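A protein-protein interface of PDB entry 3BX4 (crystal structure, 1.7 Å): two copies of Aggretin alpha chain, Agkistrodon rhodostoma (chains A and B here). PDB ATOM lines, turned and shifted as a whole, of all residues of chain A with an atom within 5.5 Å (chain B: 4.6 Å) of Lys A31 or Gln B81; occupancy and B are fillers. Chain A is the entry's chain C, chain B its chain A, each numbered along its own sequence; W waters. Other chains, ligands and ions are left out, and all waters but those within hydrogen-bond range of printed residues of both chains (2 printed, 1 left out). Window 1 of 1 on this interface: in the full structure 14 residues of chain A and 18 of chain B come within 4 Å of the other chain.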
ATOM      1  N   TRP A  26      -4.974  -8.344  15.634  1.00  0.00           N
ATOM      2  CA  TRP A  26      -4.372  -7.048  16.085  1.00  0.00           C
ATOM      3  C   TRP A  26      -4.990  -5.907  15.253  1.00  0.00           C
ATOM      4  O   TRP A  26      -5.474  -4.914  15.862  1.00  0.00           O
ATOM      5  CB  TRP A  26      -2.880  -7.129  15.985  1.00  0.00           C
ATOM      6  CG  TRP A  26      -2.159  -5.946  16.656  1.00  0.00           C
ATOM      7  CD1 TRP A  26      -1.700  -5.877  17.965  1.00  0.00           C
ATOM      8  CD2 TRP A  26      -1.955  -4.650  16.073  1.00  0.00           C
ATOM      9  NE1 TRP A  26      -1.139  -4.587  18.194  1.00  0.00           N
ATOM     10  CE2 TRP A  26      -1.320  -3.838  17.059  1.00  0.00           C
ATOM     11  CE3 TRP A  26      -2.217  -4.117  14.809  1.00  0.00           C
ATOM     12  CZ2 TRP A  26      -0.958  -2.493  16.794  1.00  0.00           C
ATOM     13  CZ3 TRP A  26      -1.878  -2.804  14.545  1.00  0.00           C
ATOM     14  CH2 TRP A  26      -1.237  -2.010  15.548  1.00  0.00           C
ATOM     15  N   ASP A  27      -4.964  -6.034  13.932  1.00  0.00           N
ATOM     16  CA  ASP A  27      -5.510  -4.975  13.037  1.00  0.00           C
ATOM     17  C   ASP A  27      -6.973  -4.702  13.280  1.00  0.00           C
ATOM     18  O   ASP A  27      -7.403  -3.545  13.360  1.00  0.00           O
ATOM     19  CB  ASP A  27      -5.287  -5.366  11.557  1.00  0.00           C
ATOM     20  CG  ASP A  27      -3.862  -5.111  11.035  1.00  0.00           C
ATOM     21  OD1 ASP A  27      -3.013  -4.316  11.570  1.00  0.00           O
ATOM     22  OD2 ASP A  27      -3.614  -5.657   9.927  1.00  0.00           O
ATOM     23  N   GLU A  28      -7.789  -5.742  13.468  1.00  0.00           N
ATOM     24  CA  GLU A  28      -9.189  -5.507  13.753  1.00  0.00           C
ATOM     25  C   GLU A  28      -9.418  -4.838  15.115  1.00  0.00           C
ATOM     26  O   GLU A  28     -10.347  -4.053  15.270  1.00  0.00           O
ATOM     27  CB  GLU A  28      -9.980  -6.847  13.745  1.00  0.00           C
ATOM     28  CG  GLU A  28     -10.125  -7.361  12.322  1.00  0.00           C
ATOM     29  CD  GLU A  28      -9.981  -6.270  11.304  1.00  0.00           C
ATOM     30  OE1 GLU A  28     -10.888  -5.419  11.255  1.00  0.00           O
ATOM     31  OE2 GLU A  28      -8.967  -6.251  10.562  1.00  0.00           O
ATOM     32  N   ALA A  29      -8.576  -5.171  16.082  1.00  0.00           N
ATOM     33  CA  ALA A  29      -8.683  -4.615  17.407  1.00  0.00           C
ATOM     34  C   ALA A  29      -8.342  -3.125  17.341  1.00  0.00           C
ATOM     35  O   ALA A  29      -9.120  -2.306  17.859  1.00  0.00           O
ATOM     36  CB  ALA A  29      -7.737  -5.331  18.341  1.00  0.00           C
ATOM     37  N   GLU A  30      -7.250  -2.808  16.682  1.00  0.00           N
ATOM     38  CA  GLU A  30      -6.883  -1.359  16.497  1.00  0.00           C
ATOM     39  C   GLU A  30      -8.003  -0.616  15.785  1.00  0.00           C
ATOM     40  O   GLU A  30      -8.369   0.488  16.193  1.00  0.00           O
ATOM     41  CB  GLU A  30      -5.534  -1.223  15.752  1.00  0.00           C
ATOM     42  CG  GLU A  30      -5.133   0.242  15.410  1.00  0.00           C
ATOM     43  CD  GLU A  30      -4.716   1.075  16.599  1.00  0.00           C
ATOM     44  OE1 GLU A  30      -4.493   0.585  17.732  1.00  0.00           O
ATOM     45  OE2 GLU A  30      -4.586   2.309  16.355  1.00  0.00           O
ATOM     46  N   LYS A  31      -8.551  -1.187  14.711  1.00  0.00           N
ATOM     47  CA  LYS A  31      -9.723  -0.578  14.001  1.00  0.00           C
ATOM     48  C   LYS A  31     -10.931  -0.358  14.906  1.00  0.00           C
ATOM     49  O   LYS A  31     -11.616   0.649  14.890  1.00  0.00           O
ATOM     50  CB  LYS A  31     -10.171  -1.420  12.753  1.00  0.00           C
ATOM     51  CG  LYS A  31      -9.152  -1.450  11.644  1.00  0.00           C
ATOM     52  CD  LYS A  31      -9.762  -1.720  10.283  1.00  0.00           C
ATOM     53  CE  LYS A  31     -10.693  -2.828  10.213  1.00  0.00           C
ATOM     54  NZ  LYS A  31     -10.775  -3.234   8.718  1.00  0.00           N
ATOM     55  N   PHE A  32     -11.254  -1.366  15.734  1.00  0.00           N
ATOM     56  CA  PHE A  32     -12.319  -1.230  16.661  1.00  0.00           C
ATOM     57  C   PHE A  32     -12.089  -0.120  17.685  1.00  0.00           C
ATOM     58  O   PHE A  32     -12.972   0.642  17.920  1.00  0.00           O
ATOM     59  CB  PHE A  32     -12.555  -2.596  17.366  1.00  0.00           C
ATOM     60  CG  PHE A  32     -13.618  -2.578  18.395  1.00  0.00           C
ATOM     61  CD1 PHE A  32     -14.922  -3.001  18.080  1.00  0.00           C
ATOM     62  CD2 PHE A  32     -13.316  -2.237  19.721  1.00  0.00           C
ATOM     63  CE1 PHE A  32     -15.911  -3.019  19.069  1.00  0.00           C
ATOM     64  CE2 PHE A  32     -14.295  -2.220  20.719  1.00  0.00           C
ATOM     65  CZ  PHE A  32     -15.615  -2.652  20.380  1.00  0.00           C
ATOM     66  N   CYS A  33     -10.849   0.018  18.181  1.00  0.00           N
ATOM     67  CA  CYS A  33     -10.595   1.060  19.114  1.00  0.00           C
ATOM     68  C   CYS A  33     -10.767   2.427  18.432  1.00  0.00           C
ATOM     69  O   CYS A  33     -11.319   3.326  19.085  1.00  0.00           O
ATOM     70  CB  CYS A  33      -9.178   0.942  19.610  1.00  0.00           C
ATOM     71  SG  CYS A  33      -8.859  -0.497  20.716  1.00  0.00           S
ATOM     72  N   ARG A  34     -10.362   2.510  17.169  1.00  0.00           N
ATOM     73  CA  ARG A  34     -10.455   3.850  16.485  1.00  0.00           C
ATOM     74  C   ARG A  34     -11.904   4.244  16.267  1.00  0.00           C
ATOM     75  O   ARG A  34     -12.271   5.381  16.126  1.00  0.00           O
ATOM     76  CB  ARG A  34      -9.777   3.814  15.108  1.00  0.00           C
ATOM     77  CG  ARG A  34      -8.342   3.545  15.135  1.00  0.00           C
ATOM     78  CD  ARG A  34      -7.596   4.874  15.523  1.00  0.00           C
ATOM     79  NE  ARG A  34      -7.892   6.057  14.620  1.00  0.00           N
ATOM     80  CZ  ARG A  34      -7.148   6.394  13.536  1.00  0.00           C
ATOM     81  NH1 ARG A  34      -6.148   5.636  13.123  1.00  0.00           N
ATOM     82  NH2 ARG A  34      -7.432   7.494  12.782  1.00  0.00           N
ATOM     83  N   ALA A  35     -12.828   3.234  16.303  1.00  0.00           N
ATOM     84  CA  ALA A  35     -14.235   3.507  16.177  1.00  0.00           C
ATOM     85  C   ALA A  35     -14.963   3.833  17.496  1.00  0.00           C
ATOM     86  O   ALA A  35     -16.192   4.102  17.500  1.00  0.00           O
ATOM     87  CB  ALA A  35     -14.897   2.319  15.482  1.00  0.00           C
ATOM     88  N   LYS B  79       1.036   3.483   7.498  1.00  0.00           N
ATOM     89  CA  LYS B  79       0.395   2.610   8.478  1.00  0.00           C
ATOM     90  C   LYS B  79      -1.126   2.709   8.613  1.00  0.00           C
ATOM     91  O   LYS B  79      -1.771   1.779   9.107  1.00  0.00           O
ATOM     92  CB  LYS B  79       0.993   2.893   9.853  1.00  0.00           C
ATOM     93  N   GLU B  80      -1.711   3.840   8.209  1.00  0.00           N
ATOM     94  CA  GLU B  80      -3.137   4.060   8.348  1.00  0.00           C
ATOM     95  C   GLU B  80      -3.939   3.184   7.415  1.00  0.00           C
ATOM     96  O   GLU B  80      -3.458   2.810   6.340  1.00  0.00           O
ATOM     97  CB  GLU B  80      -3.480   5.559   8.094  1.00  0.00           C
ATOM     98  CG  GLU B  80      -2.825   6.514   9.115  1.00  0.00           C
ATOM     99  CD  GLU B  80      -3.397   6.373  10.515  1.00  0.00           C
ATOM    100  OE1 GLU B  80      -4.579   5.968  10.666  1.00  0.00           O
ATOM    101  OE2 GLU B  80      -2.677   6.688  11.477  1.00  0.00           O
ATOM    102  N   GLN B  81      -5.166   2.867   7.839  1.00  0.00           N
ATOM    103  CA  GLN B  81      -6.111   2.045   7.058  1.00  0.00           C
ATOM    104  C   GLN B  81      -6.734   2.764   5.852  1.00  0.00           C
ATOM    105  O   GLN B  81      -7.301   2.143   4.946  1.00  0.00           O
ATOM    106  CB  GLN B  81      -7.211   1.581   7.982  1.00  0.00           C
ATOM    107  CG  GLN B  81      -6.722   0.538   8.938  1.00  0.00           C
ATOM    108  CD  GLN B  81      -6.618  -0.789   8.229  1.00  0.00           C
ATOM    109  OE1 GLN B  81      -5.581  -1.448   8.256  1.00  0.00           O
ATOM    110  NE2 GLN B  81      -7.700  -1.161   7.532  1.00  0.00           N
ATOM    111  N   GLN B  82      -6.677   4.101   5.849  1.00  0.00           N
ATOM    112  CA  GLN B  82      -7.071   4.874   4.697  1.00  0.00           C
ATOM    113  C   GLN B  82      -6.154   6.092   4.797  1.00  0.00           C
ATOM    114  O   GLN B  82      -5.768   6.479   5.907  1.00  0.00           O
ATOM    115  CB  GLN B  82      -8.596   5.174   4.648  1.00  0.00           C
ATOM    116  CG  GLN B  82      -9.210   5.994   5.775  1.00  0.00           C
ATOM    117  CD  GLN B  82      -8.850   7.488   5.618  1.00  0.00           C
ATOM    118  OE1 GLN B  82      -8.635   7.943   4.497  1.00  0.00           O
ATOM    119  NE2 GLN B  82      -8.831   8.218   6.719  1.00  0.00           N
ATOM    120  N   CYS B  83      -5.791   6.635   3.655  1.00  0.00           N
ATOM    121  CA  CYS B  83      -4.603   7.506   3.609  1.00  0.00           C
ATOM    122  C   CYS B  83      -4.922   8.978   3.569  1.00  0.00           C
ATOM    123  O   CYS B  83      -3.999   9.771   3.295  1.00  0.00           O
ATOM    124  CB  CYS B  83      -3.728   7.170   2.405  1.00  0.00           C
ATOM    125  SG  CYS B  83      -3.259   5.410   2.432  1.00  0.00           S
ATOM    126  N   GLU B  96     -12.672   6.978  13.366  1.00  0.00           N
ATOM    127  CA  GLU B  96     -13.055   6.478  12.053  1.00  0.00           C
ATOM    128  C   GLU B  96     -13.704   5.119  12.293  1.00  0.00           C
ATOM    129  O   GLU B  96     -13.364   4.441  13.273  1.00  0.00           O
ATOM    130  CB  GLU B  96     -11.911   6.429  11.032  1.00  0.00           C
ATOM    131  CG  GLU B  96     -10.648   5.960  11.534  1.00  0.00           C
ATOM    132  CD  GLU B  96      -9.534   5.821  10.515  1.00  0.00           C
ATOM    133  OE1 GLU B  96      -9.393   6.626   9.538  1.00  0.00           O
ATOM    134  OE2 GLU B  96      -8.710   4.959  10.794  1.00  0.00           O
ATOM    135  N   LEU B  98     -13.934   1.946  10.478  1.00  0.00           N
ATOM    136  CA  LEU B  98     -13.521   1.107   9.326  1.00  0.00           C
ATOM    137  C   LEU B  98     -13.675  -0.367   9.652  1.00  0.00           C
ATOM    138  O   LEU B  98     -13.070  -1.199   9.013  1.00  0.00           O
ATOM    139  CB  LEU B  98     -12.064   1.390   8.921  1.00  0.00           C
ATOM    140  CG  LEU B  98     -11.801   2.866   8.478  1.00  0.00           C
ATOM    141  CD1 LEU B  98     -10.290   2.939   8.267  1.00  0.00           C
ATOM    142  CD2 LEU B  98     -12.592   3.112   7.256  1.00  0.00           C
ATOM    143  N   ILE B  99     -14.490  -0.643  10.660  1.00  0.00           N
ATOM    144  CA  ILE B  99     -14.693  -2.020  11.154  1.00  0.00           C
ATOM    145  C   ILE B  99     -15.098  -3.058  10.050  1.00  0.00           C
ATOM    146  O   ILE B  99     -14.533  -4.166  10.024  1.00  0.00           O
ATOM    147  CB  ILE B  99     -15.680  -2.017  12.317  1.00  0.00           C
ATOM    148  CG1 ILE B  99     -15.037  -1.421  13.589  1.00  0.00           C
ATOM    149  CG2 ILE B  99     -16.095  -3.479  12.666  1.00  0.00           C
ATOM    150  CD1 ILE B  99     -16.086  -1.151  14.644  1.00  0.00           C
ATOM    151  N   LEU B 101     -14.790  -2.793   6.736  1.00  0.00           N
ATOM    152  CA  LEU B 101     -14.149  -2.440   5.507  1.00  0.00           C
ATOM    153  C   LEU B 101     -12.724  -2.986   5.462  1.00  0.00           C
ATOM    154  O   LEU B 101     -11.999  -2.873   6.434  1.00  0.00           O
ATOM    155  CB  LEU B 101     -14.115  -0.930   5.412  1.00  0.00           C
ATOM    156  CG  LEU B 101     -14.274  -0.420   3.991  1.00  0.00           C
ATOM    157  CD1 LEU B 101     -15.588  -1.023   3.406  1.00  0.00           C
ATOM    158  CD2 LEU B 101     -14.267   1.101   4.045  1.00  0.00           C
ATOM    159  N   THR B 103      -8.984  -2.737   3.708  1.00  0.00           N
ATOM    160  CA  THR B 103      -8.125  -1.740   3.091  1.00  0.00           C
ATOM    161  C   THR B 103      -7.540  -2.271   1.773  1.00  0.00           C
ATOM    162  O   THR B 103      -7.523  -3.481   1.564  1.00  0.00           O
ATOM    163  CB  THR B 103      -7.011  -1.310   4.103  1.00  0.00           C
ATOM    164  OG1 THR B 103      -6.428  -0.087   3.640  1.00  0.00           O
ATOM    165  CG2 THR B 103      -5.931  -2.398   4.254  1.00  0.00           C
ATOM    166  N   LYS B 105      -4.204  -1.834   0.105  1.00  0.00           N
ATOM    167  CA  LYS B 105      -2.842  -1.306   0.270  1.00  0.00           C
ATOM    168  C   LYS B 105      -1.762  -2.086  -0.457  1.00  0.00           C
ATOM    169  O   LYS B 105      -0.540  -1.919  -0.187  1.00  0.00           O
ATOM    170  CB  LYS B 105      -2.578  -1.253   1.757  1.00  0.00           C
ATOM    171  CG  LYS B 105      -3.341  -0.077   2.370  1.00  0.00           C
ATOM    172  CD  LYS B 105      -3.167   0.061   3.873  1.00  0.00           C
ATOM    173  CE  LYS B 105      -1.915   0.829   4.222  1.00  0.00           C
ATOM    174  NZ  LYS B 105      -1.725   0.776   5.689  1.00  0.00           N
HETATM  175  O   HOH W   1     -11.959   2.078  12.617  1.00  0.00           O
HETATM  176  O   HOH W   2      -5.923   3.590  10.520  1.00  0.00           O
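NZ of Lys A31 is in hydrogen-bond range of O of Leu B98 (3.1 Å).
OE1 of Glu B80 lies within salt-bridge range of NH1 of Arg A34.
The side-chain carboxylate (OE2) of Glu B96 is in salt-bridge range of the guanidinium group (NH2) of Arg A34, at 3.5 Å.
The backbone carbonyl oxygen (O) of Glu B96 sits close to the backbone NH (N) of Ala A35 (3.3 Å).
The side-chain amino group of Lys A31 sits at hydrogen-bond distance from the backbone carbonyl oxygen of Leu B101, at 2.6 Å.
NE2 of Gln B82 lies within hydrogen-bond range of OE1 of Glu B96, 3.3 Å away.
The side-chain carboxylate (OE1) of Glu A28 is in salt-bridge range of the side-chain amino group (NZ) of Lys A31 (3.4 Å).
The side-chain hydroxyl (OG1) of Thr B103 lies within hydrogen-bond range of the backbone carbonyl oxygen (O) of Gln B81 (2.7 Å).
NZ of Lys B105 sits at hydrogen-bond distance from O of Glu B80, 2.8 Å away.
Among the printed residues, pairs that only touch across the chains: Lys A31 with Gln B81 and Ala A35 with Ile B99.
Gln B81 touches just one residue of chain A: Lys A31 (3.5 Å).
Of the printed residues of chain A, Leu B98 touches Lys A31.
Printed residues of chain A within 4 Å of Glu B96: Arg A34 and Ala A35.
Of the printed residues of chain A, Leu B101 touches Lys A31.
Ala A29 touches none of the printed residues of chain B.
The nearest residue of chain A that does not touch Gln B81 is Asp A27 (4.9 Å).
Of the 10 printed residues of chain A, 3 touch a printed residue of chain B.
Printed residues of chain A that touch a printed residue of chain B: Lys A31, Arg A34 and Ala A35.
Hydrophobic or aromatic side chains of chain A within 4 Å of the printed part of chain B: Ala A35.
Printed residues of chain B that touch a printed residue of chain A: Glu B80, Gln B81, Glu B96, Leu B98, Ile B99 and Leu B101.
Hydrophobic or aromatic side chains of chain B that line the printed part of chain A: Ile B99.
Among the printed residues, Asp or Glu carboxylates within 4 Å of a Lys or Arg side-chain nitrogen of the other chain: Arg A34 with Glu B80 and Arg A34 with Glu B96.
No position is printed for both chains.
Of the 7 pairs that touch across the chains among the printed residues, none has its exchanged pair printed and touching as well.
Water W1 lies within hydrogen-bond range of the backbone carbonyl oxygen (O) of Lys A31 (2.7 Å), the backbone carbonyl oxygen (O) of Glu B96 (2.8 Å) and the backbone NH (N) of Leu B98 (2.9 Å).
Water W2 lies within hydrogen-bond range of OE1 of Glu B80 (2.7 Å), N of Gln B81 (2.9 Å), OE2 of Glu B96 (3.1 Å) and NH1 of Arg A34 (3.3 Å).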
